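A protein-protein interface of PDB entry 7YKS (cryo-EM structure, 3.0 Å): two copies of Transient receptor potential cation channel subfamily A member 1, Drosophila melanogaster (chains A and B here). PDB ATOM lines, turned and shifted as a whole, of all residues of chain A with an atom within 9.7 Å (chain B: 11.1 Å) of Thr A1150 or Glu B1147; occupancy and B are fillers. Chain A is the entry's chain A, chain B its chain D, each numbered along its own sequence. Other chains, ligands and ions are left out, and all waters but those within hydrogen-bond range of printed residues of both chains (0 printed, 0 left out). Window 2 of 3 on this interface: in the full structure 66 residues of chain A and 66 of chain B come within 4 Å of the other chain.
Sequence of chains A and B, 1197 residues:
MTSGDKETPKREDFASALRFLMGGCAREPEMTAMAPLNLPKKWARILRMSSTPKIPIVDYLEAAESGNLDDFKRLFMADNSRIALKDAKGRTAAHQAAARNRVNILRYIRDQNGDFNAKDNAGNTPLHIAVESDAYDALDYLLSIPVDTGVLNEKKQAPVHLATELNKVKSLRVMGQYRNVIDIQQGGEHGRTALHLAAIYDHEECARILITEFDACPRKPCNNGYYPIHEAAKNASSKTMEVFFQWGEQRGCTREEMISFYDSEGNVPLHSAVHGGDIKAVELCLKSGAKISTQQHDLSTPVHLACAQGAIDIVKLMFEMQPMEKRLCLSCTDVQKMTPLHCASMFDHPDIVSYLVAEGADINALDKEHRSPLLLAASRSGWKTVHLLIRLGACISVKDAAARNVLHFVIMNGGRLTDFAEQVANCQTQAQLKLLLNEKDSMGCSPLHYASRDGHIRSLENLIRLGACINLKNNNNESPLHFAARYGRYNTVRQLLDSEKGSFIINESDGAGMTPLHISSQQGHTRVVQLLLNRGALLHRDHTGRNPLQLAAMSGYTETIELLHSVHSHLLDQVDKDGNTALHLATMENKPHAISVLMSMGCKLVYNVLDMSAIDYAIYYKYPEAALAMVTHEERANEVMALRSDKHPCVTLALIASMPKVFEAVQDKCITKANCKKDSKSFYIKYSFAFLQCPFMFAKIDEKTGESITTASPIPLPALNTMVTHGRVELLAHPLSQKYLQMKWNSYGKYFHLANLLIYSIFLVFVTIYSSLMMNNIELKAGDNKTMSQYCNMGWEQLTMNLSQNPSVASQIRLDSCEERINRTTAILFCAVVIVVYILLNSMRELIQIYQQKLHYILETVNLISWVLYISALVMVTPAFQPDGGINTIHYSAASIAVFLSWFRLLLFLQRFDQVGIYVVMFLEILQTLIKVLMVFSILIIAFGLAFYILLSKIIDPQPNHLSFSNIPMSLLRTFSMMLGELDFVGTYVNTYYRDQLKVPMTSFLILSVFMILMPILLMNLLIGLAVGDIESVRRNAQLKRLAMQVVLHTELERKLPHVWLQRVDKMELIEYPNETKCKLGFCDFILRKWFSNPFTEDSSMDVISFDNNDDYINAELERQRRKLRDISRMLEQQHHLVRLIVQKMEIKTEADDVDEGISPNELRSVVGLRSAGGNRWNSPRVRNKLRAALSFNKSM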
ATOM      1  N   ILE A1142       2.141   2.009   0.480  1.00  0.00           N
ATOM      2  CA  ILE A1142       1.237   2.983  -0.128  1.00  0.00           C
ATOM      3  C   ILE A1142       0.433   3.706   0.941  1.00  0.00           C
ATOM      4  O   ILE A1142       0.353   4.934   0.943  1.00  0.00           O
ATOM      5  CB  ILE A1142       0.321   2.301  -1.159  1.00  0.00           C
ATOM      6  CG1 ILE A1142       1.131   1.803  -2.347  1.00  0.00           C
ATOM      7  CG2 ILE A1142      -0.749   3.248  -1.642  1.00  0.00           C
ATOM      8  CD1 ILE A1142       0.373   0.882  -3.254  1.00  0.00           C
ATOM      9  N   MET A1146       0.283   7.689   1.293  1.00  0.00           N
ATOM     10  CA  MET A1146      -0.859   8.101   0.496  1.00  0.00           C
ATOM     11  C   MET A1146      -1.351   9.461   0.963  1.00  0.00           C
ATOM     12  O   MET A1146      -1.351   9.761   2.159  1.00  0.00           O
ATOM     13  CB  MET A1146      -1.973   7.060   0.610  1.00  0.00           C
ATOM     14  CG  MET A1146      -3.206   7.297  -0.196  1.00  0.00           C
ATOM     15  SD  MET A1146      -4.266   5.870  -0.038  1.00  0.00           S
ATOM     16  CE  MET A1146      -4.597   5.914   1.708  1.00  0.00           C
ATOM     17  N   GLU A1147      -1.767  10.284   0.008  1.00  0.00           N
ATOM     18  CA  GLU A1147      -2.310  11.601   0.300  1.00  0.00           C
ATOM     19  C   GLU A1147      -3.783  11.460   0.660  1.00  0.00           C
ATOM     20  O   GLU A1147      -4.560  10.909  -0.123  1.00  0.00           O
ATOM     21  CB  GLU A1147      -2.129  12.505  -0.916  1.00  0.00           C
ATOM     22  CG  GLU A1147      -2.382  13.962  -0.666  1.00  0.00           C
ATOM     23  CD  GLU A1147      -1.283  14.593   0.155  1.00  0.00           C
ATOM     24  OE1 GLU A1147      -0.142  14.090   0.094  1.00  0.00           O
ATOM     25  OE2 GLU A1147      -1.553  15.585   0.859  1.00  0.00           O
ATOM     26  N   ILE A1148      -4.170  11.939   1.841  1.00  0.00           N
ATOM     27  CA  ILE A1148      -5.549  11.856   2.318  1.00  0.00           C
ATOM     28  C   ILE A1148      -5.999  13.260   2.696  1.00  0.00           C
ATOM     29  O   ILE A1148      -5.550  13.809   3.710  1.00  0.00           O
ATOM     30  CB  ILE A1148      -5.698  10.899   3.508  1.00  0.00           C
ATOM     31  CG1 ILE A1148      -5.345   9.471   3.112  1.00  0.00           C
ATOM     32  CG2 ILE A1148      -7.113  10.922   4.042  1.00  0.00           C
ATOM     33  CD1 ILE A1148      -5.283   8.540   4.280  1.00  0.00           C
ATOM     34  N   LYS A1149      -6.865  13.852   1.876  1.00  0.00           N
ATOM     35  CA  LYS A1149      -7.415  15.173   2.157  1.00  0.00           C
ATOM     36  C   LYS A1149      -8.929  15.187   2.288  1.00  0.00           C
ATOM     37  O   LYS A1149      -9.454  15.646   3.308  1.00  0.00           O
ATOM     38  CB  LYS A1149      -6.978  16.160   1.068  1.00  0.00           C
ATOM     39  CG  LYS A1149      -5.499  16.469   1.084  1.00  0.00           C
ATOM     40  CD  LYS A1149      -5.145  17.222   2.347  1.00  0.00           C
ATOM     41  CE  LYS A1149      -3.698  17.650   2.371  1.00  0.00           C
ATOM     42  NZ  LYS A1149      -3.360  18.349   3.636  1.00  0.00           N
ATOM     43  N   THR A1150      -9.649  14.689   1.285  1.00  0.00           N
ATOM     44  CA  THR A1150     -11.105  14.774   1.285  1.00  0.00           C
ATOM     45  C   THR A1150     -11.724  13.770   2.246  1.00  0.00           C
ATOM     46  O   THR A1150     -12.681  14.092   2.961  1.00  0.00           O
ATOM     47  CB  THR A1150     -11.631  14.554  -0.133  1.00  0.00           C
ATOM     48  OG1 THR A1150     -11.088  15.558  -0.997  1.00  0.00           O
ATOM     49  CG2 THR A1150     -13.144  14.632  -0.186  1.00  0.00           C
ATOM     50  N   GLU A1151     -11.171  12.563   2.306  1.00  0.00           N
ATOM     51  CA  GLU A1151     -11.718  11.502   3.132  1.00  0.00           C
ATOM     52  C   GLU A1151     -11.055  11.425   4.497  1.00  0.00           C
ATOM     53  O   GLU A1151     -11.096  10.372   5.138  1.00  0.00           O
ATOM     54  CB  GLU A1151     -11.603  10.171   2.399  1.00  0.00           C
ATOM     55  CG  GLU A1151     -12.445  10.114   1.142  1.00  0.00           C
ATOM     56  CD  GLU A1151     -13.927  10.120   1.434  1.00  0.00           C
ATOM     57  OE1 GLU A1151     -14.332   9.548   2.467  1.00  0.00           O
ATOM     58  OE2 GLU A1151     -14.689  10.700   0.638  1.00  0.00           O
ATOM     59  N   ALA A1152     -10.459  12.520   4.961  1.00  0.00           N
ATOM     60  CA  ALA A1152      -9.878  12.560   6.292  1.00  0.00           C
ATOM     61  C   ALA A1152     -10.970  12.708   7.337  1.00  0.00           C
ATOM     62  O   ALA A1152     -11.936  13.452   7.147  1.00  0.00           O
ATOM     63  CB  ALA A1152      -8.886  13.713   6.409  1.00  0.00           C
ATOM     64  N   ASP A1153     -10.816  11.995   8.444  1.00  0.00           N
ATOM     65  CA  ASP A1153     -11.783  12.045   9.531  1.00  0.00           C
ATOM     66  C   ASP A1153     -11.710  13.373  10.275  1.00  0.00           C
ATOM     67  O   ASP A1153     -12.727  14.037  10.483  1.00  0.00           O
ATOM     68  CB  ASP A1153     -11.549  10.888  10.498  1.00  0.00           C
ATOM     69  CG  ASP A1153     -11.884   9.546   9.888  1.00  0.00           C
ATOM     70  OD1 ASP A1153     -12.796   9.492   9.037  1.00  0.00           O
ATOM     71  OD2 ASP A1153     -11.226   8.546  10.246  1.00  0.00           O
ATOM     72  N   ASN B 477     -16.256   6.353  14.631  1.00  0.00           N
ATOM     73  CA  ASN B 477     -14.923   5.861  14.254  1.00  0.00           C
ATOM     74  C   ASN B 477     -13.832   5.951  15.328  1.00  0.00           C
ATOM     75  O   ASN B 477     -14.130   6.143  16.500  1.00  0.00           O
ATOM     76  CB  ASN B 477     -14.443   6.527  12.959  1.00  0.00           C
ATOM     77  CG  ASN B 477     -15.203   6.055  11.725  1.00  0.00           C
ATOM     78  OD1 ASN B 477     -15.780   4.968  11.719  1.00  0.00           O
ATOM     79  ND2 ASN B 477     -15.187   6.860  10.666  1.00  0.00           N
ATOM     80  N   PHE B 483      -5.564   6.032  14.208  1.00  0.00           N
ATOM     81  CA  PHE B 483      -5.492   5.759  12.779  1.00  0.00           C
ATOM     82  C   PHE B 483      -4.063   5.870  12.279  1.00  0.00           C
ATOM     83  O   PHE B 483      -3.599   5.027  11.507  1.00  0.00           O
ATOM     84  CB  PHE B 483      -6.395   6.717  12.001  1.00  0.00           C
ATOM     85  CG  PHE B 483      -6.412   6.461  10.517  1.00  0.00           C
ATOM     86  CD1 PHE B 483      -7.169   5.431   9.992  1.00  0.00           C
ATOM     87  CD2 PHE B 483      -5.664   7.242   9.651  1.00  0.00           C
ATOM     88  CE1 PHE B 483      -7.182   5.190   8.638  1.00  0.00           C
ATOM     89  CE2 PHE B 483      -5.671   7.000   8.300  1.00  0.00           C
ATOM     90  CZ  PHE B 483      -6.431   5.977   7.794  1.00  0.00           C
ATOM     91  N   ARG B 489       2.599   6.127   8.725  1.00  0.00           N
ATOM     92  CA  ARG B 489       2.009   7.469   8.774  1.00  0.00           C
ATOM     93  C   ARG B 489       2.734   8.356   9.798  1.00  0.00           C
ATOM     94  O   ARG B 489       2.203   8.747  10.834  1.00  0.00           O
ATOM     95  CB  ARG B 489       0.503   7.333   9.039  1.00  0.00           C
ATOM     96  CG  ARG B 489      -0.355   8.573   8.958  1.00  0.00           C
ATOM     97  CD  ARG B 489      -0.467   9.177   7.573  1.00  0.00           C
ATOM     98  NE  ARG B 489      -1.193   8.353   6.621  1.00  0.00           N
ATOM     99  CZ  ARG B 489      -1.323   8.670   5.341  1.00  0.00           C
ATOM    100  NH1 ARG B 489      -0.795   9.791   4.882  1.00  0.00           N
ATOM    101  NH2 ARG B 489      -1.989   7.879   4.522  1.00  0.00           N
ATOM    102  N   VAL B1139      -5.822  -2.888   0.580  1.00  0.00           N
ATOM    103  CA  VAL B1139      -6.223  -2.451  -0.758  1.00  0.00           C
ATOM    104  C   VAL B1139      -7.620  -1.852  -0.718  1.00  0.00           C
ATOM    105  O   VAL B1139      -7.909  -0.842  -1.370  1.00  0.00           O
ATOM    106  CB  VAL B1139      -6.141  -3.638  -1.739  1.00  0.00           C
ATOM    107  CG1 VAL B1139      -6.624  -3.254  -3.103  1.00  0.00           C
ATOM    108  CG2 VAL B1139      -4.734  -4.147  -1.834  1.00  0.00           C
ATOM    109  N   LEU B1141      -8.820  -0.401   1.899  1.00  0.00           N
ATOM    110  CA  LEU B1141      -8.713   0.867   2.608  1.00  0.00           C
ATOM    111  C   LEU B1141      -8.260   1.989   1.689  1.00  0.00           C
ATOM    112  O   LEU B1141      -8.661   3.141   1.886  1.00  0.00           O
ATOM    113  CB  LEU B1141      -7.735   0.738   3.774  1.00  0.00           C
ATOM    114  CG  LEU B1141      -7.571   1.961   4.674  1.00  0.00           C
ATOM    115  CD1 LEU B1141      -8.825   2.207   5.476  1.00  0.00           C
ATOM    116  CD2 LEU B1141      -6.375   1.845   5.555  1.00  0.00           C
ATOM    117  N   ILE B1142      -7.426   1.674   0.694  1.00  0.00           N
ATOM    118  CA  ILE B1142      -6.877   2.694  -0.198  1.00  0.00           C
ATOM    119  C   ILE B1142      -7.987   3.365  -0.991  1.00  0.00           C
ATOM    120  O   ILE B1142      -8.058   4.592  -1.055  1.00  0.00           O
ATOM    121  CB  ILE B1142      -5.810   2.083  -1.123  1.00  0.00           C
ATOM    122  CG1 ILE B1142      -4.594   1.643  -0.321  1.00  0.00           C
ATOM    123  CG2 ILE B1142      -5.383   3.071  -2.181  1.00  0.00           C
ATOM    124  CD1 ILE B1142      -3.637   0.786  -1.091  1.00  0.00           C
ATOM    125  N   VAL B1143      -8.921   2.575  -1.528  1.00  0.00           N
ATOM    126  CA  VAL B1143     -10.013   3.145  -2.310  1.00  0.00           C
ATOM    127  C   VAL B1143     -11.021   3.896  -1.447  1.00  0.00           C
ATOM    128  O   VAL B1143     -11.837   4.650  -1.982  1.00  0.00           O
ATOM    129  CB  VAL B1143     -10.732   2.055  -3.123  1.00  0.00           C
ATOM    130  CG1 VAL B1143      -9.777   1.389  -4.075  1.00  0.00           C
ATOM    131  CG2 VAL B1143     -11.344   1.036  -2.211  1.00  0.00           C
ATOM    132  N   GLN B1144     -10.995   3.715  -0.126  1.00  0.00           N
ATOM    133  CA  GLN B1144     -11.851   4.516   0.739  1.00  0.00           C
ATOM    134  C   GLN B1144     -11.288   5.905   0.963  1.00  0.00           C
ATOM    135  O   GLN B1144     -12.045   6.833   1.251  1.00  0.00           O
ATOM    136  CB  GLN B1144     -12.029   3.856   2.101  1.00  0.00           C
ATOM    137  CG  GLN B1144     -12.770   2.563   2.106  1.00  0.00           C
ATOM    138  CD  GLN B1144     -12.931   2.033   3.508  1.00  0.00           C
ATOM    139  OE1 GLN B1144     -12.477   2.655   4.466  1.00  0.00           O
ATOM    140  NE2 GLN B1144     -13.560   0.873   3.639  1.00  0.00           N
ATOM    141  N   LYS B1145      -9.969   6.057   0.874  1.00  0.00           N
ATOM    142  CA  LYS B1145      -9.304   7.302   1.233  1.00  0.00           C
ATOM    143  C   LYS B1145      -8.372   7.793   0.135  1.00  0.00           C
ATOM    144  O   LYS B1145      -7.480   8.600   0.400  1.00  0.00           O
ATOM    145  CB  LYS B1145      -8.546   7.130   2.546  1.00  0.00           C
ATOM    146  CG  LYS B1145      -9.465   6.951   3.727  1.00  0.00           C
ATOM    147  CD  LYS B1145      -8.718   6.788   5.013  1.00  0.00           C
ATOM    148  CE  LYS B1145      -9.695   6.591   6.141  1.00  0.00           C
ATOM    149  NZ  LYS B1145     -10.473   7.828   6.382  1.00  0.00           N
ATOM    150  N   MET B1146      -8.566   7.322  -1.090  1.00  0.00           N
ATOM    151  CA  MET B1146      -7.795   7.794  -2.226  1.00  0.00           C
ATOM    152  C   MET B1146      -8.340   9.131  -2.701  1.00  0.00           C
ATOM    153  O   MET B1146      -9.550   9.363  -2.696  1.00  0.00           O
ATOM    154  CB  MET B1146      -7.851   6.763  -3.354  1.00  0.00           C
ATOM    155  CG  MET B1146      -7.061   7.061  -4.584  1.00  0.00           C
ATOM    156  SD  MET B1146      -7.138   5.642  -5.663  1.00  0.00           S
ATOM    157  CE  MET B1146      -8.885   5.590  -5.991  1.00  0.00           C
ATOM    158  N   GLU B1147      -7.434  10.013  -3.105  1.00  0.00           N
ATOM    159  CA  GLU B1147      -7.800  11.319  -3.631  1.00  0.00           C
ATOM    160  C   GLU B1147      -8.154  11.176  -5.105  1.00  0.00           C
ATOM    161  O   GLU B1147      -7.342  10.681  -5.890  1.00  0.00           O
ATOM    162  CB  GLU B1147      -6.638  12.287  -3.440  1.00  0.00           C
ATOM    163  CG  GLU B1147      -6.971  13.731  -3.673  1.00  0.00           C
ATOM    164  CD  GLU B1147      -7.825  14.300  -2.566  1.00  0.00           C
ATOM    165  OE1 GLU B1147      -7.734  13.787  -1.431  1.00  0.00           O
ATOM    166  OE2 GLU B1147      -8.585  15.253  -2.822  1.00  0.00           O
ATOM    167  N   ILE B1148      -9.360  11.591  -5.486  1.00  0.00           N
ATOM    168  CA  ILE B1148      -9.835  11.499  -6.866  1.00  0.00           C
ATOM    169  C   ILE B1148     -10.292  12.886  -7.297  1.00  0.00           C
ATOM    170  O   ILE B1148     -11.334  13.369  -6.841  1.00  0.00           O
ATOM    171  CB  ILE B1148     -10.968  10.478  -7.027  1.00  0.00           C
ATOM    172  CG1 ILE B1148     -10.491   9.071  -6.692  1.00  0.00           C
ATOM    173  CG2 ILE B1148     -11.504  10.489  -8.441  1.00  0.00           C
ATOM    174  CD1 ILE B1148     -11.603   8.074  -6.643  1.00  0.00           C
ATOM    175  N   LYS B1149      -9.508  13.535  -8.156  1.00  0.00           N
ATOM    176  CA  LYS B1149      -9.865  14.845  -8.689  1.00  0.00           C
ATOM    177  C   LYS B1149      -9.999  14.871 -10.203  1.00  0.00           C
ATOM    178  O   LYS B1149     -11.044  15.278 -10.721  1.00  0.00           O
ATOM    179  CB  LYS B1149      -8.833  15.886  -8.239  1.00  0.00           C
ATOM    180  CG  LYS B1149      -8.866  16.175  -6.756  1.00  0.00           C
ATOM    181  CD  LYS B1149     -10.169  16.849  -6.391  1.00  0.00           C
ATOM    182  CE  LYS B1149     -10.215  17.257  -4.939  1.00  0.00           C
ATOM    183  NZ  LYS B1149     -11.518  17.878  -4.592  1.00  0.00           N
ATOM    184  N   THR B1150      -8.970  14.440 -10.930  1.00  0.00           N
ATOM    185  CA  THR B1150      -8.977  14.543 -12.384  1.00  0.00           C
ATOM    186  C   THR B1150      -9.880  13.495 -13.016  1.00  0.00           C
ATOM    187  O   THR B1150     -10.613  13.787 -13.968  1.00  0.00           O
ATOM    188  CB  THR B1150      -7.549  14.412 -12.913  1.00  0.00           C
ATOM    189  OG1 THR B1150      -6.743  15.456 -12.358  1.00  0.00           O
ATOM    190  CG2 THR B1150      -7.503  14.513 -14.426  1.00  0.00           C
ATOM    191  N   GLU B1151      -9.870  12.279 -12.479  1.00  0.00           N
ATOM    192  CA  GLU B1151     -10.634  11.180 -13.038  1.00  0.00           C
ATOM    193  C   GLU B1151     -11.992  11.017 -12.375  1.00  0.00           C
ATOM    194  O   GLU B1151     -12.572   9.930 -12.430  1.00  0.00           O
ATOM    195  CB  GLU B1151      -9.827   9.891 -12.942  1.00  0.00           C
ATOM    196  CG  GLU B1151      -8.569   9.918 -13.785  1.00  0.00           C
ATOM    197  CD  GLU B1151      -8.863   9.926 -15.266  1.00  0.00           C
ATOM    198  OE1 GLU B1151      -9.862   9.301 -15.678  1.00  0.00           O
ATOM    199  OE2 GLU B1151      -8.103  10.561 -16.021  1.00  0.00           O
ATOM    200  N   ALA B1152     -12.517  12.075 -11.765  1.00  0.00           N
ATOM    201  CA  ALA B1152     -13.847  12.032 -11.183  1.00  0.00           C
ATOM    202  C   ALA B1152     -14.901  12.134 -12.273  1.00  0.00           C
ATOM    203  O   ALA B1152     -14.755  12.901 -13.229  1.00  0.00           O
ATOM    204  CB  ALA B1152     -14.028  13.163 -10.177  1.00  0.00           C
ATOM    205  N   ASP B1153     -15.965  11.357 -12.127  1.00  0.00           N
ATOM    206  CA  ASP B1153     -17.054  11.357 -13.093  1.00  0.00           C
ATOM    207  C   ASP B1153     -17.873  12.640 -13.002  1.00  0.00           C
ATOM    208  O   ASP B1153     -18.120  13.303 -14.010  1.00  0.00           O
ATOM    209  CB  ASP B1153     -17.953  10.143 -12.874  1.00  0.00           C
ATOM    210  CG  ASP B1153     -17.268   8.844 -13.227  1.00  0.00           C
ATOM    211  OD1 ASP B1153     -16.417   8.851 -14.140  1.00  0.00           O
ATOM    212  OD2 ASP B1153     -17.567   7.816 -12.583  1.00  0.00           O
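The backbone carbonyl oxygen (O) of Met A1146 is in hydrogen-bond range of the guanidinium group (NH1) of Arg B489. The backbone NH (N) of Lys A1149 is in hydrogen-bond range of the side-chain carboxylate (OE1) of Glu B1147, at 3.4 Å. The backbone carbonyl oxygen (O) of Glu A1151 is in hydrogen-bond range of the side-chain amino group (NZ) of Lys B1145 (2.9 Å). The side-chain hydroxyl of Thr A1150 sits at hydrogen-bond distance from the side-chain carboxylate of Glu B1147 (3.1 Å). The side-chain amino group (NZ) of Lys B1145 is in salt-bridge range of the side-chain carboxylate (OD1) of Asp A1153 (3.9 Å).
Printed residues of chain B within 4 Å of Lys A1149: Glu B1147 (3.4 Å). Printed residues of chain B within 4 Å of Asp A1153: Asn B477 (3.9 Å) and Lys B1145 (3.9 Å). Leu B1141 touches none of the printed residues of chain A. Of the printed residues of chain A, Gln B1144 touches Glu A1151. No residue of chain A comes within 4 Å of Met B1146. Glu B1147 touches two residues of chain A. No residue of chain A comes within 4 Å of Ile B1148. Asp B1153 touches none of the printed residues of chain A. The nearest residue of chain B that does not touch Thr A1150 is Lys B1149 (4.3 Å). The nearest residue of chain A that does not touch Glu B1147 is Glu A1147 (4.1 Å).
Of the 17 printed residues of chain B, 6 touch a printed residue of chain A. Printed residues of chain B that touch a printed residue of chain A: Asn B477, Arg B489, Ile B1142, Gln B1144, Lys B1145 and Glu B1147. Hydrophobic or aromatic side chains of chain B within 4 Å of the printed part of chain A: Ile B1142. Of the 9 printed residues of chain A, 8 touch a printed residue of chain B. Among the printed residues, 12 pairs touch across the chains.
Among the printed residues, merely in contact across the chains: Ile A1142 with Ile B1142 (3.8 Å), Met A1146 with Ile B1142 (3.7 Å), Glu A1147 with Lys B1145 (3.8 Å), Ile A1148 with Arg B489 (3.4 Å), Ile A1148 with Lys B1145 (3.6 Å), Glu A1151 with Gln B1144 (3.3 Å) and Asp A1153 with Asn B477 (3.9 Å).
Ile B1142 touches its own counterpart, Ile A1142. Met A1146 touches Ile B1142, but with the chains exchanged Ile A1142 does not touch Met B1146 (7.9 Å). Lys A1149 touches Glu B1147, but with the chains exchanged Glu A1147 does not touch Lys B1149 (9.2 Å). Thr A1150 touches Glu B1147, but with the chains exchanged Glu A1147 does not touch Thr B1150 (12.2 Å). Of the 12 pairs that touch across the chains among the printed residues, 1 has its exchanged pair printed and touching as well.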
